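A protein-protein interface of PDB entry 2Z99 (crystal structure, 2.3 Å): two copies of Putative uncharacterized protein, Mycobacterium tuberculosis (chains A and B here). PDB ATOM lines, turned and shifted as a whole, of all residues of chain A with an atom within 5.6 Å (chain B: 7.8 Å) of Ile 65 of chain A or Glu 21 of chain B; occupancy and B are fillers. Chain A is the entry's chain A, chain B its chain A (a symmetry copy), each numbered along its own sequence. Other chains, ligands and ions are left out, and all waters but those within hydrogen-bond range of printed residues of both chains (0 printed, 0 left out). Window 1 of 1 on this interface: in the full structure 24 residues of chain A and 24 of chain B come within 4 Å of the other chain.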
ATOM      1  N   LEU A  58     -18.948  22.630  -4.836  1.00  0.00           N
ATOM      2  CA  LEU A  58     -18.206  21.368  -4.774  1.00  0.00           C
ATOM      3  C   LEU A  58     -16.713  21.565  -4.953  1.00  0.00           C
ATOM      4  O   LEU A  58     -15.918  20.996  -4.208  1.00  0.00           O
ATOM      5  CB  LEU A  58     -18.732  20.388  -5.825  1.00  0.00           C
ATOM      6  CG  LEU A  58     -20.162  19.929  -5.503  1.00  0.00           C
ATOM      7  CD1 LEU A  58     -20.765  19.180  -6.683  1.00  0.00           C
ATOM      8  CD2 LEU A  58     -20.139  19.063  -4.236  1.00  0.00           C
ATOM      9  N   THR A  59     -16.311  22.375  -5.925  1.00  0.00           N
ATOM     10  CA  THR A  59     -14.880  22.578  -6.105  1.00  0.00           C
ATOM     11  C   THR A  59     -14.398  23.599  -5.103  1.00  0.00           C
ATOM     12  O   THR A  59     -13.207  23.825  -4.944  1.00  0.00           O
ATOM     13  CB  THR A  59     -14.522  23.001  -7.553  1.00  0.00           C
ATOM     14  OG1 THR A  59     -13.637  24.124  -7.532  1.00  0.00           O
ATOM     15  CG2 THR A  59     -15.740  23.321  -8.320  1.00  0.00           C
ATOM     16  N   ARG A  61     -15.003  23.182  -1.976  1.00  0.00           N
ATOM     17  CA  ARG A  61     -14.582  22.362  -0.848  1.00  0.00           C
ATOM     18  C   ARG A  61     -13.745  21.183  -1.300  1.00  0.00           C
ATOM     19  O   ARG A  61     -13.483  20.259  -0.531  1.00  0.00           O
ATOM     20  CB  ARG A  61     -15.788  21.868  -0.044  1.00  0.00           C
ATOM     21  CG  ARG A  61     -16.807  21.040  -0.779  1.00  0.00           C
ATOM     22  CD  ARG A  61     -17.981  20.829   0.159  1.00  0.00           C
ATOM     23  NE  ARG A  61     -19.006  19.930  -0.369  1.00  0.00           N
ATOM     24  CZ  ARG A  61     -18.866  18.612  -0.501  1.00  0.00           C
ATOM     25  NH1 ARG A  61     -17.734  18.001  -0.145  1.00  0.00           N
ATOM     26  NH2 ARG A  61     -19.872  17.901  -0.990  1.00  0.00           N
ATOM     27  N   ASP A  62     -13.321  21.239  -2.559  1.00  0.00           N
ATOM     28  CA  ASP A  62     -12.495  20.201  -3.145  1.00  0.00           C
ATOM     29  C   ASP A  62     -13.152  18.849  -2.943  1.00  0.00           C
ATOM     30  O   ASP A  62     -12.508  17.884  -2.522  1.00  0.00           O
ATOM     31  CB  ASP A  62     -11.109  20.214  -2.503  1.00  0.00           C
ATOM     32  CG  ASP A  62     -10.051  19.660  -3.422  1.00  0.00           C
ATOM     33  OD1 ASP A  62     -10.358  19.469  -4.614  1.00  0.00           O
ATOM     34  OD2 ASP A  62      -8.909  19.433  -2.975  1.00  0.00           O
ATOM     35  N   SER A  63     -14.440  18.782  -3.253  1.00  0.00           N
ATOM     36  CA  SER A  63     -15.180  17.551  -3.079  1.00  0.00           C
ATOM     37  C   SER A  63     -14.621  16.397  -3.915  1.00  0.00           C
ATOM     38  O   SER A  63     -13.851  16.607  -4.856  1.00  0.00           O
ATOM     39  CB  SER A  63     -16.649  17.771  -3.429  1.00  0.00           C
ATOM     40  OG  SER A  63     -17.367  16.565  -3.250  1.00  0.00           O
ATOM     41  N   GLY A  64     -14.996  15.173  -3.547  1.00  0.00           N
ATOM     42  CA  GLY A  64     -14.557  14.015  -4.305  1.00  0.00           C
ATOM     43  C   GLY A  64     -15.346  14.022  -5.606  1.00  0.00           C
ATOM     44  O   GLY A  64     -14.918  13.487  -6.633  1.00  0.00           O
ATOM     45  N   ILE A  65     -16.508  14.658  -5.549  1.00  0.00           N
ATOM     46  CA  ILE A  65     -17.403  14.784  -6.688  1.00  0.00           C
ATOM     47  C   ILE A  65     -17.207  16.126  -7.394  1.00  0.00           C
ATOM     48  O   ILE A  65     -17.166  17.186  -6.751  1.00  0.00           O
ATOM     49  CB  ILE A  65     -18.875  14.668  -6.240  1.00  0.00           C
ATOM     50  CG1 ILE A  65     -19.106  13.317  -5.562  1.00  0.00           C
ATOM     51  CG2 ILE A  65     -19.800  14.840  -7.436  1.00  0.00           C
ATOM     52  CD1 ILE A  65     -20.490  13.155  -4.964  1.00  0.00           C
ATOM     53  N   ASP A  66     -17.077  16.072  -8.717  1.00  0.00           N
ATOM     54  CA  ASP A  66     -16.889  17.270  -9.523  1.00  0.00           C
ATOM     55  C   ASP A  66     -17.952  17.328 -10.610  1.00  0.00           C
ATOM     56  O   ASP A  66     -17.945  16.517 -11.542  1.00  0.00           O
ATOM     57  CB  ASP A  66     -15.512  17.275 -10.177  1.00  0.00           C
ATOM     58  CG  ASP A  66     -15.245  18.552 -10.942  1.00  0.00           C
ATOM     59  OD1 ASP A  66     -16.143  19.410 -10.971  1.00  0.00           O
ATOM     60  OD2 ASP A  66     -14.145  18.710 -11.508  1.00  0.00           O
ATOM     61  N   LEU A  67     -18.863  18.291 -10.475  1.00  0.00           N
ATOM     62  CA  LEU A  67     -19.946  18.484 -11.427  1.00  0.00           C
ATOM     63  C   LEU A  67     -19.383  19.278 -12.595  1.00  0.00           C
ATOM     64  O   LEU A  67     -19.014  20.439 -12.441  1.00  0.00           O
ATOM     65  CB  LEU A  67     -21.095  19.242 -10.757  1.00  0.00           C
ATOM     66  CG  LEU A  67     -22.387  19.509 -11.532  1.00  0.00           C
ATOM     67  CD1 LEU A  67     -23.045  18.212 -12.010  1.00  0.00           C
ATOM     68  CD2 LEU A  67     -23.331  20.268 -10.622  1.00  0.00           C
ATOM     69  N   MET A  76     -22.016  14.399 -12.953  1.00  0.00           N
ATOM     70  CA  MET A  76     -21.107  14.348 -11.810  1.00  0.00           C
ATOM     71  C   MET A  76     -19.928  13.427 -12.127  1.00  0.00           C
ATOM     72  O   MET A  76     -20.122  12.261 -12.475  1.00  0.00           O
ATOM     73  CB  MET A  76     -21.819  13.815 -10.570  1.00  0.00           C
ATOM     74  CG  MET A  76     -22.938  14.689 -10.087  1.00  0.00           C
ATOM     75  SD  MET A  76     -23.361  14.360  -8.404  1.00  0.00           S
ATOM     76  CE  MET A  76     -24.583  13.106  -8.625  1.00  0.00           C
ATOM     77  N   TYR A  77     -18.714  13.955 -12.011  1.00  0.00           N
ATOM     78  CA  TYR A  77     -17.500  13.191 -12.267  1.00  0.00           C
ATOM     79  C   TYR A  77     -16.655  13.060 -10.998  1.00  0.00           C
ATOM     80  O   TYR A  77     -16.879  13.745  -9.998  1.00  0.00           O
ATOM     81  CB  TYR A  77     -16.626  13.883 -13.323  1.00  0.00           C
ATOM     82  CG  TYR A  77     -17.254  14.008 -14.688  1.00  0.00           C
ATOM     83  CD1 TYR A  77     -18.450  14.698 -14.862  1.00  0.00           C
ATOM     84  CD2 TYR A  77     -16.669  13.405 -15.803  1.00  0.00           C
ATOM     85  CE1 TYR A  77     -19.059  14.784 -16.111  1.00  0.00           C
ATOM     86  CE2 TYR A  77     -17.269  13.484 -17.063  1.00  0.00           C
ATOM     87  CZ  TYR A  77     -18.465  14.172 -17.209  1.00  0.00           C
ATOM     88  OH  TYR A  77     -19.085  14.232 -18.436  1.00  0.00           O
ATOM     89  N   THR A  78     -15.676  12.166 -11.056  1.00  0.00           N
ATOM     90  CA  THR A  78     -14.735  11.969  -9.965  1.00  0.00           C
ATOM     91  C   THR A  78     -13.691  13.078 -10.135  1.00  0.00           C
ATOM     92  O   THR A  78     -13.165  13.279 -11.234  1.00  0.00           O
ATOM     93  CB  THR A  78     -14.064  10.603 -10.081  1.00  0.00           C
ATOM     94  OG1 THR A  78     -14.755   9.671  -9.242  1.00  0.00           O
ATOM     95  CG2 THR A  78     -12.585  10.686  -9.707  1.00  0.00           C
ATOM     96  N   ARG A  79     -13.401  13.809  -9.066  1.00  0.00           N
ATOM     97  CA  ARG A  79     -12.432  14.893  -9.159  1.00  0.00           C
ATOM     98  C   ARG A  79     -11.056  14.314  -9.461  1.00  0.00           C
ATOM     99  O   ARG A  79     -10.626  13.339  -8.840  1.00  0.00           O
ATOM    100  CB  ARG A  79     -12.429  15.714  -7.862  1.00  0.00           C
ATOM    101  CG  ARG A  79     -11.820  17.100  -8.006  1.00  0.00           C
ATOM    102  CD  ARG A  79     -12.102  17.985  -6.784  1.00  0.00           C
ATOM    103  NE  ARG A  79     -13.513  18.367  -6.665  1.00  0.00           N
ATOM    104  CZ  ARG A  79     -14.097  19.336  -7.363  1.00  0.00           C
ATOM    105  NH1 ARG A  79     -13.402  20.048  -8.237  1.00  0.00           N
ATOM    106  NH2 ARG A  79     -15.387  19.581  -7.204  1.00  0.00           N
ATOM    107  N   ASP B  14     -11.365  15.523   6.765  1.00  0.00           N
ATOM    108  CA  ASP B  14     -11.820  16.147   5.532  1.00  0.00           C
ATOM    109  C   ASP B  14     -11.322  15.471   4.258  1.00  0.00           C
ATOM    110  O   ASP B  14     -12.017  15.476   3.251  1.00  0.00           O
ATOM    111  CB  ASP B  14     -11.439  17.634   5.531  1.00  0.00           C
ATOM    112  CG  ASP B  14     -12.428  18.485   6.307  1.00  0.00           C
ATOM    113  OD1 ASP B  14     -13.298  17.907   6.996  1.00  0.00           O
ATOM    114  OD2 ASP B  14     -12.337  19.727   6.224  1.00  0.00           O
ATOM    115  N   GLU B  15     -10.130  14.893   4.283  1.00  0.00           N
ATOM    116  CA  GLU B  15      -9.634  14.214   3.090  1.00  0.00           C
ATOM    117  C   GLU B  15     -10.340  12.881   2.894  1.00  0.00           C
ATOM    118  O   GLU B  15     -10.772  12.558   1.801  1.00  0.00           O
ATOM    119  CB  GLU B  15      -8.127  13.985   3.172  1.00  0.00           C
ATOM    120  CG  GLU B  15      -7.338  15.050   2.473  1.00  0.00           C
ATOM    121  CD  GLU B  15      -7.717  15.177   1.012  1.00  0.00           C
ATOM    122  OE1 GLU B  15      -7.471  14.217   0.251  1.00  0.00           O
ATOM    123  OE2 GLU B  15      -8.268  16.236   0.625  1.00  0.00           O
ATOM    124  N   LEU B  16     -10.469  12.118   3.969  1.00  0.00           N
ATOM    125  CA  LEU B  16     -11.126  10.816   3.915  1.00  0.00           C
ATOM    126  C   LEU B  16     -12.536  10.982   3.359  1.00  0.00           C
ATOM    127  O   LEU B  16     -13.004  10.156   2.571  1.00  0.00           O
ATOM    128  CB  LEU B  16     -11.207  10.205   5.315  1.00  0.00           C
ATOM    129  CG  LEU B  16     -11.088   8.683   5.478  1.00  0.00           C
ATOM    130  CD1 LEU B  16     -12.204   8.192   6.394  1.00  0.00           C
ATOM    131  CD2 LEU B  16     -11.146   7.990   4.137  1.00  0.00           C
ATOM    132  N   LYS B  17     -13.209  12.051   3.776  1.00  0.00           N
ATOM    133  CA  LYS B  17     -14.561  12.315   3.315  1.00  0.00           C
ATOM    134  C   LYS B  17     -14.560  12.525   1.803  1.00  0.00           C
ATOM    135  O   LYS B  17     -15.447  12.047   1.101  1.00  0.00           O
ATOM    136  CB  LYS B  17     -15.135  13.540   4.031  1.00  0.00           C
ATOM    137  CG  LYS B  17     -16.555  13.909   3.619  1.00  0.00           C
ATOM    138  CD  LYS B  17     -17.303  14.544   4.791  1.00  0.00           C
ATOM    139  CE  LYS B  17     -18.664  15.100   4.390  1.00  0.00           C
ATOM    140  NZ  LYS B  17     -18.551  16.403   3.675  1.00  0.00           N
ATOM    141  N   ARG B  18     -13.548  13.226   1.307  1.00  0.00           N
ATOM    142  CA  ARG B  18     -13.446  13.489  -0.121  1.00  0.00           C
ATOM    143  C   ARG B  18     -13.256  12.198  -0.893  1.00  0.00           C
ATOM    144  O   ARG B  18     -14.044  11.879  -1.782  1.00  0.00           O
ATOM    145  CB  ARG B  18     -12.278  14.426  -0.398  1.00  0.00           C
ATOM    146  CG  ARG B  18     -12.411  15.755   0.305  1.00  0.00           C
ATOM    147  CD  ARG B  18     -11.271  16.669  -0.055  1.00  0.00           C
ATOM    148  NE  ARG B  18     -11.516  18.005   0.461  1.00  0.00           N
ATOM    149  CZ  ARG B  18     -10.844  18.556   1.465  1.00  0.00           C
ATOM    150  NH1 ARG B  18      -9.866  17.891   2.071  1.00  0.00           N
ATOM    151  NH2 ARG B  18     -11.163  19.775   1.866  1.00  0.00           N
ATOM    152  N   VAL B  19     -12.207  11.455  -0.561  1.00  0.00           N
ATOM    153  CA  VAL B  19     -11.939  10.197  -1.226  1.00  0.00           C
ATOM    154  C   VAL B  19     -13.209   9.331  -1.239  1.00  0.00           C
ATOM    155  O   VAL B  19     -13.595   8.812  -2.285  1.00  0.00           O
ATOM    156  CB  VAL B  19     -10.802   9.430  -0.518  1.00  0.00           C
ATOM    157  CG1 VAL B  19     -10.522   8.136  -1.248  1.00  0.00           C
ATOM    158  CG2 VAL B  19      -9.542  10.279  -0.479  1.00  0.00           C
ATOM    159  N   LEU B  20     -13.879   9.202  -0.095  1.00  0.00           N
ATOM    160  CA  LEU B  20     -15.085   8.386  -0.031  1.00  0.00           C
ATOM    161  C   LEU B  20     -16.201   8.888  -0.946  1.00  0.00           C
ATOM    162  O   LEU B  20     -17.027   8.096  -1.413  1.00  0.00           O
ATOM    163  CB  LEU B  20     -15.597   8.274   1.411  1.00  0.00           C
ATOM    164  CG  LEU B  20     -14.709   7.453   2.361  1.00  0.00           C
ATOM    165  CD1 LEU B  20     -15.347   7.346   3.758  1.00  0.00           C
ATOM    166  CD2 LEU B  20     -14.503   6.059   1.775  1.00  0.00           C
ATOM    167  N   GLU B  21     -16.233  10.194  -1.195  1.00  0.00           N
ATOM    168  CA  GLU B  21     -17.250  10.758  -2.072  1.00  0.00           C
ATOM    169  C   GLU B  21     -16.941  10.306  -3.501  1.00  0.00           C
ATOM    170  O   GLU B  21     -17.817   9.876  -4.230  1.00  0.00           O
ATOM    171  CB  GLU B  21     -17.249  12.299  -2.017  1.00  0.00           C
ATOM    172  CG  GLU B  21     -17.722  12.909  -0.699  1.00  0.00           C
ATOM    173  CD  GLU B  21     -17.756  14.431  -0.734  1.00  0.00           C
ATOM    174  OE1 GLU B  21     -16.760  15.052  -1.167  1.00  0.00           O
ATOM    175  OE2 GLU B  21     -18.783  15.006  -0.320  1.00  0.00           O
ATOM    176  N   ALA B  22     -15.679  10.417  -3.893  1.00  0.00           N
ATOM    177  CA  ALA B  22     -15.265  10.021  -5.224  1.00  0.00           C
ATOM    178  C   ALA B  22     -15.596   8.551  -5.465  1.00  0.00           C
ATOM    179  O   ALA B  22     -16.134   8.205  -6.515  1.00  0.00           O
ATOM    180  CB  ALA B  22     -13.778  10.255  -5.395  1.00  0.00           C
ATOM    181  N   LEU B  23     -15.300   7.702  -4.483  1.00  0.00           N
ATOM    182  CA  LEU B  23     -15.530   6.268  -4.595  1.00  0.00           C
ATOM    183  C   LEU B  23     -16.998   5.892  -4.611  1.00  0.00           C
ATOM    184  O   LEU B  23     -17.427   5.082  -5.435  1.00  0.00           O
ATOM    185  CB  LEU B  23     -14.802   5.516  -3.465  1.00  0.00           C
ATOM    186  CG  LEU B  23     -13.298   5.808  -3.327  1.00  0.00           C
ATOM    187  CD1 LEU B  23     -12.714   5.048  -2.145  1.00  0.00           C
ATOM    188  CD2 LEU B  23     -12.575   5.437  -4.608  1.00  0.00           C
ATOM    189  N   LEU B  24     -17.779   6.474  -3.713  1.00  0.00           N
ATOM    190  CA  LEU B  24     -19.200   6.173  -3.667  1.00  0.00           C
ATOM    191  C   LEU B  24     -19.887   6.590  -4.963  1.00  0.00           C
ATOM    192  O   LEU B  24     -21.021   6.184  -5.231  1.00  0.00           O
ATOM    193  CB  LEU B  24     -19.867   6.908  -2.509  1.00  0.00           C
ATOM    194  CG  LEU B  24     -19.595   6.402  -1.097  1.00  0.00           C
ATOM    195  CD1 LEU B  24     -20.219   7.366  -0.094  1.00  0.00           C
ATOM    196  CD2 LEU B  24     -20.165   4.993  -0.944  1.00  0.00           C
ATOM    197  N   LEU B  25     -19.199   7.400  -5.761  1.00  0.00           N
ATOM    198  CA  LEU B  25     -19.771   7.891  -7.010  1.00  0.00           C
ATOM    199  C   LEU B  25     -19.654   6.905  -8.162  1.00  0.00           C
ATOM    200  O   LEU B  25     -20.631   6.659  -8.867  1.00  0.00           O
ATOM    201  CB  LEU B  25     -19.105   9.222  -7.418  1.00  0.00           C
ATOM    202  CG  LEU B  25     -19.640   9.902  -8.688  1.00  0.00           C
ATOM    203  CD1 LEU B  25     -20.979  10.570  -8.389  1.00  0.00           C
ATOM    204  CD2 LEU B  25     -18.640  10.933  -9.203  1.00  0.00           C
ATOM    205  N   VAL B  26     -18.468   6.328  -8.337  1.00  0.00           N
ATOM    206  CA  VAL B  26     -18.201   5.395  -9.429  1.00  0.00           C
ATOM    207  C   VAL B  26     -18.773   3.972  -9.347  1.00  0.00           C
ATOM    208  O   VAL B  26     -18.784   3.254 -10.349  1.00  0.00           O
ATOM    209  CB  VAL B  26     -16.689   5.255  -9.679  1.00  0.00           C
ATOM    210  CG1 VAL B  26     -16.460   4.856 -11.108  1.00  0.00           C
ATOM    211  CG2 VAL B  26     -15.981   6.548  -9.401  1.00  0.00           C
ATOM    212  N   ILE B  27     -19.250   3.559  -8.180  1.00  0.00           N
ATOM    213  CA  ILE B  27     -19.776   2.202  -8.039  1.00  0.00           C
ATOM    214  C   ILE B  27     -21.184   2.027  -8.592  1.00  0.00           C
ATOM    215  O   ILE B  27     -22.021   2.928  -8.490  1.00  0.00           O
ATOM    216  CB  ILE B  27     -19.784   1.756  -6.569  1.00  0.00           C
ATOM    217  CG1 ILE B  27     -20.723   2.651  -5.764  1.00  0.00           C
ATOM    218  CG2 ILE B  27     -18.368   1.769  -6.026  1.00  0.00           C
ATOM    219  CD1 ILE B  27     -20.882   2.257  -4.337  1.00  0.00           C
ATOM    220  N   LEU B  36     -13.810  -0.239   0.768  1.00  0.00           N
ATOM    221  CA  LEU B  36     -13.448   1.171   0.830  1.00  0.00           C
ATOM    222  C   LEU B  36     -12.216   1.304   1.723  1.00  0.00           C
ATOM    223  O   LEU B  36     -11.230   1.943   1.352  1.00  0.00           O
ATOM    224  CB  LEU B  36     -14.632   1.979   1.382  1.00  0.00           C
ATOM    225  CG  LEU B  36     -15.809   2.065   0.395  1.00  0.00           C
ATOM    226  CD1 LEU B  36     -16.999   2.720   1.025  1.00  0.00           C
ATOM    227  CD2 LEU B  36     -15.375   2.841  -0.829  1.00  0.00           C
ATOM    228  N   LYS B  50     -17.117   7.060   9.342  1.00  0.00           N
ATOM    229  CA  LYS B  50     -17.193   8.177   8.415  1.00  0.00           C
ATOM    230  C   LYS B  50     -18.427   8.120   7.509  1.00  0.00           C
ATOM    231  O   LYS B  50     -19.117   9.133   7.298  1.00  0.00           O
ATOM    232  CB  LYS B  50     -15.934   8.201   7.560  1.00  0.00           C
ATOM    233  CG  LYS B  50     -15.940   9.283   6.511  1.00  0.00           C
ATOM    234  CD  LYS B  50     -14.835  10.282   6.761  1.00  0.00           C
ATOM    235  CE  LYS B  50     -15.110  11.121   7.986  1.00  0.00           C
ATOM    236  NZ  LYS B  50     -16.145  12.137   7.678  1.00  0.00           N
ATOM    237  N   LEU B  51     -18.702   6.932   6.979  1.00  0.00           N
ATOM    238  CA  LEU B  51     -19.836   6.743   6.090  1.00  0.00           C
ATOM    239  C   LEU B  51     -21.127   7.058   6.823  1.00  0.00           C
ATOM    240  O   LEU B  51     -22.045   7.654   6.250  1.00  0.00           O
ATOM    241  CB  LEU B  51     -19.839   5.311   5.560  1.00  0.00           C
ATOM    242  CG  LEU B  51     -18.714   4.980   4.569  1.00  0.00           C
ATOM    243  CD1 LEU B  51     -18.527   3.483   4.465  1.00  0.00           C
ATOM    244  CD2 LEU B  51     -19.044   5.573   3.199  1.00  0.00           C
ATOM    245  N   MET B  54     -21.225  10.840   7.160  1.00  0.00           N
ATOM    246  CA  MET B  54     -21.562  11.449   5.873  1.00  0.00           C
ATOM    247  C   MET B  54     -23.043  11.193   5.593  1.00  0.00           C
ATOM    248  O   MET B  54     -23.729  12.045   5.043  1.00  0.00           O
ATOM    249  CB  MET B  54     -20.717  10.841   4.756  1.00  0.00           C
ATOM    250  CG  MET B  54     -19.242  11.117   4.902  1.00  0.00           C
ATOM    251  SD  MET B  54     -18.255  10.210   3.724  1.00  0.00           S
ATOM    252  CE  MET B  54     -19.028  10.814   2.152  1.00  0.00           C
ATOM    253  N   GLU B  57     -24.981  13.643   7.796  1.00  0.00           N
ATOM    254  CA  GLU B  57     -24.958  15.013   7.285  1.00  0.00           C
ATOM    255  C   GLU B  57     -25.939  15.189   6.119  1.00  0.00           C
ATOM    256  O   GLU B  57     -26.699  16.158   6.083  1.00  0.00           O
ATOM    257  CB  GLU B  57     -23.553  15.370   6.801  1.00  0.00           C
ATOM    258  CG  GLU B  57     -22.471  15.202   7.832  1.00  0.00           C
ATOM    259  CD  GLU B  57     -21.080  15.240   7.219  1.00  0.00           C
ATOM    260  OE1 GLU B  57     -20.964  15.548   6.015  1.00  0.00           O
ATOM    261  OE2 GLU B  57     -20.100  14.966   7.947  1.00  0.00           O
ATOM    262  N   LEU B  58     -25.911  14.255   5.167  1.00  0.00           N
ATOM    263  CA  LEU B  58     -26.793  14.314   4.000  1.00  0.00           C
ATOM    264  C   LEU B  58     -28.260  14.340   4.384  1.00  0.00           C
ATOM    265  O   LEU B  58     -29.029  15.133   3.847  1.00  0.00           O
ATOM    266  CB  LEU B  58     -26.521  13.133   3.066  1.00  0.00           C
ATOM    267  CG  LEU B  58     -25.133  13.236   2.415  1.00  0.00           C
ATOM    268  CD1 LEU B  58     -24.771  11.935   1.713  1.00  0.00           C
ATOM    269  CD2 LEU B  58     -25.118  14.425   1.447  1.00  0.00           C
ATOM    270  N   ARG B  61     -29.394  17.624   5.911  1.00  0.00           N
ATOM    271  CA  ARG B  61     -29.782  18.730   5.046  1.00  0.00           C
ATOM    272  C   ARG B  61     -30.808  18.299   4.019  1.00  0.00           C
ATOM    273  O   ARG B  61     -31.094  19.023   3.065  1.00  0.00           O
ATOM    274  CB  ARG B  61     -28.563  19.335   4.344  1.00  0.00           C
ATOM    275  CG  ARG B  61     -27.749  18.417   3.474  1.00  0.00           C
ATOM    276  CD  ARG B  61     -26.510  19.179   3.043  1.00  0.00           C
ATOM    277  NE  ARG B  61     -25.675  18.459   2.084  1.00  0.00           N
ATOM    278  CZ  ARG B  61     -25.995  18.246   0.808  1.00  0.00           C
ATOM    279  NH1 ARG B  61     -27.146  18.695   0.303  1.00  0.00           N
ATOM    280  NH2 ARG B  61     -25.151  17.581   0.033  1.00  0.00           N
ATOM    281  N   ILE B  65     -29.404  13.250  -2.368  1.00  0.00           N
ATOM    282  CA  ILE B  65     -28.639  12.019  -2.244  1.00  0.00           C
ATOM    283  C   ILE B  65     -28.744  11.449  -0.830  1.00  0.00           C
ATOM    284  O   ILE B  65     -28.576  12.170   0.164  1.00  0.00           O
ATOM    285  CB  ILE B  65     -27.151  12.268  -2.571  1.00  0.00           C
ATOM    286  CG1 ILE B  65     -27.016  12.806  -3.996  1.00  0.00           C
ATOM    287  CG2 ILE B  65     -26.357  10.981  -2.398  1.00  0.00           C
ATOM    288  CD1 ILE B  65     -25.603  13.211  -4.371  1.00  0.00           C
ATOM    289  N   MET B  76     -24.870   5.211  -2.591  1.00  0.00           N
ATOM    290  CA  MET B  76     -25.639   6.452  -2.639  1.00  0.00           C
ATOM    291  C   MET B  76     -26.954   6.218  -3.384  1.00  0.00           C
ATOM    292  O   MET B  76     -26.951   5.760  -4.529  1.00  0.00           O
ATOM    293  CB  MET B  76     -24.862   7.548  -3.362  1.00  0.00           C
ATOM    294  CG  MET B  76     -23.593   7.951  -2.671  1.00  0.00           C
ATOM    295  SD  MET B  76     -23.022   9.537  -3.199  1.00  0.00           S
ATOM    296  CE  MET B  76     -22.002   9.068  -4.561  1.00  0.00           C
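The backbone carbonyl oxygen (O) of Asp 62 of chain A sits close to the guanidinium group (NE) of Arg 18 of chain B (3.1 Å).
The backbone carbonyl oxygen (O) of Ala 22 of chain B lies within hydrogen-bond range of the side-chain hydroxyl (OG1) of Thr 78 of chain A (3.4 Å).
The guanidinium group (NE) of Arg 18 of chain B is in hydrogen-bond range of the backbone carbonyl oxygen (O) of Arg 61 of chain A.
OE2 of Glu 21 of chain B is in salt-bridge range of NH2 of Arg 61 of chain A (3.2 Å).
The side-chain hydroxyl of Ser 63 of chain A sits at hydrogen-bond distance from the side-chain carboxylate of Glu 21 of chain B (2.6 Å).
The backbone NH (N) of Gly 64 of chain A sits at hydrogen-bond distance from the side-chain carboxylate (OE1) of Glu 21 of chain B, at 3.0 Å.
The backbone carbonyl oxygen (O) of Tyr 77 of chain A is in hydrogen-bond range of the backbone NH (N) of Asp 66 of chain A, at 2.7 Å.
The backbone carbonyl oxygen (O) of Asp 14 of chain B sits close to the guanidinium group (NH1) of Arg 18 of chain B, at 3.4 Å.
The backbone carbonyl oxygen of Leu 58 of chain A sits at hydrogen-bond distance from the backbone NH of Ser 63 of chain A, 2.8 Å away.
The side-chain carboxylate of Asp 62 of chain A is in salt-bridge range of the guanidinium group of Arg 79 of chain A.
The side-chain carboxylate (OE2) of Glu 15 of chain B is in salt-bridge range of the guanidinium group (NH1) of Arg 18 of chain B (2.7 Å).
The backbone carbonyl oxygen (O) of Ser 63 of chain A sits at hydrogen-bond distance from the guanidinium group (NE) of Arg 79 of chain A (2.5 Å).
Among the printed residues, merely in contact across the chains: Gly 64 of chain A with Arg 18 of chain B, Gly 64 of chain A with Ala 22 of chain B, Ile 65 of chain A with Glu 21 of chain B, Met 76 of chain A with Leu 25 of chain B, Tyr 77 of chain A with Leu 25 of chain B, Thr 78 of chain A with Leu 25 of chain B and Thr 78 of chain A with Val 26 of chain B.
Ile 65 of chain A touches just one residue of chain B: Glu 21.
Glu 21 of chain B touches just these residues of chain A: Arg 61, Ser 63, Gly 64 and Ile 65.
Of the printed residues of chain A, Val 26 of chain B touches Thr 78 (3.4 Å).
Printed residues of chain B within 4 Å of Tyr 77 of chain A: Leu 25.
Leu 24 of chain B touches none of the printed residues of chain A.
Of the 13 printed residues of chain A, 8 touch a printed residue of chain B.
Printed residues of chain A that touch a printed residue of chain B: Arg 61, Asp 62, Ser 63, Gly 64, Ile 65, Met 76, Tyr 77 and Thr 78.
Of the 23 printed residues of chain B, 5 touch a printed residue of chain A.
Printed residues of chain B that touch a printed residue of chain A: Arg 18, Glu 21, Ala 22, Leu 25 and Val 26.
Along chain B the printed residues that touch a printed residue of chain A span positions 18 to 26.
Among the printed residues, 13 pairs touch across the chains.
Among the printed residues, Asp or Glu carboxylates within 4 Å of a Lys or Arg side-chain nitrogen of the other chain: Arg 61 of chain A with Glu 21 of chain B.
Positions printed for both chains: 58, 61, 65 and 76.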
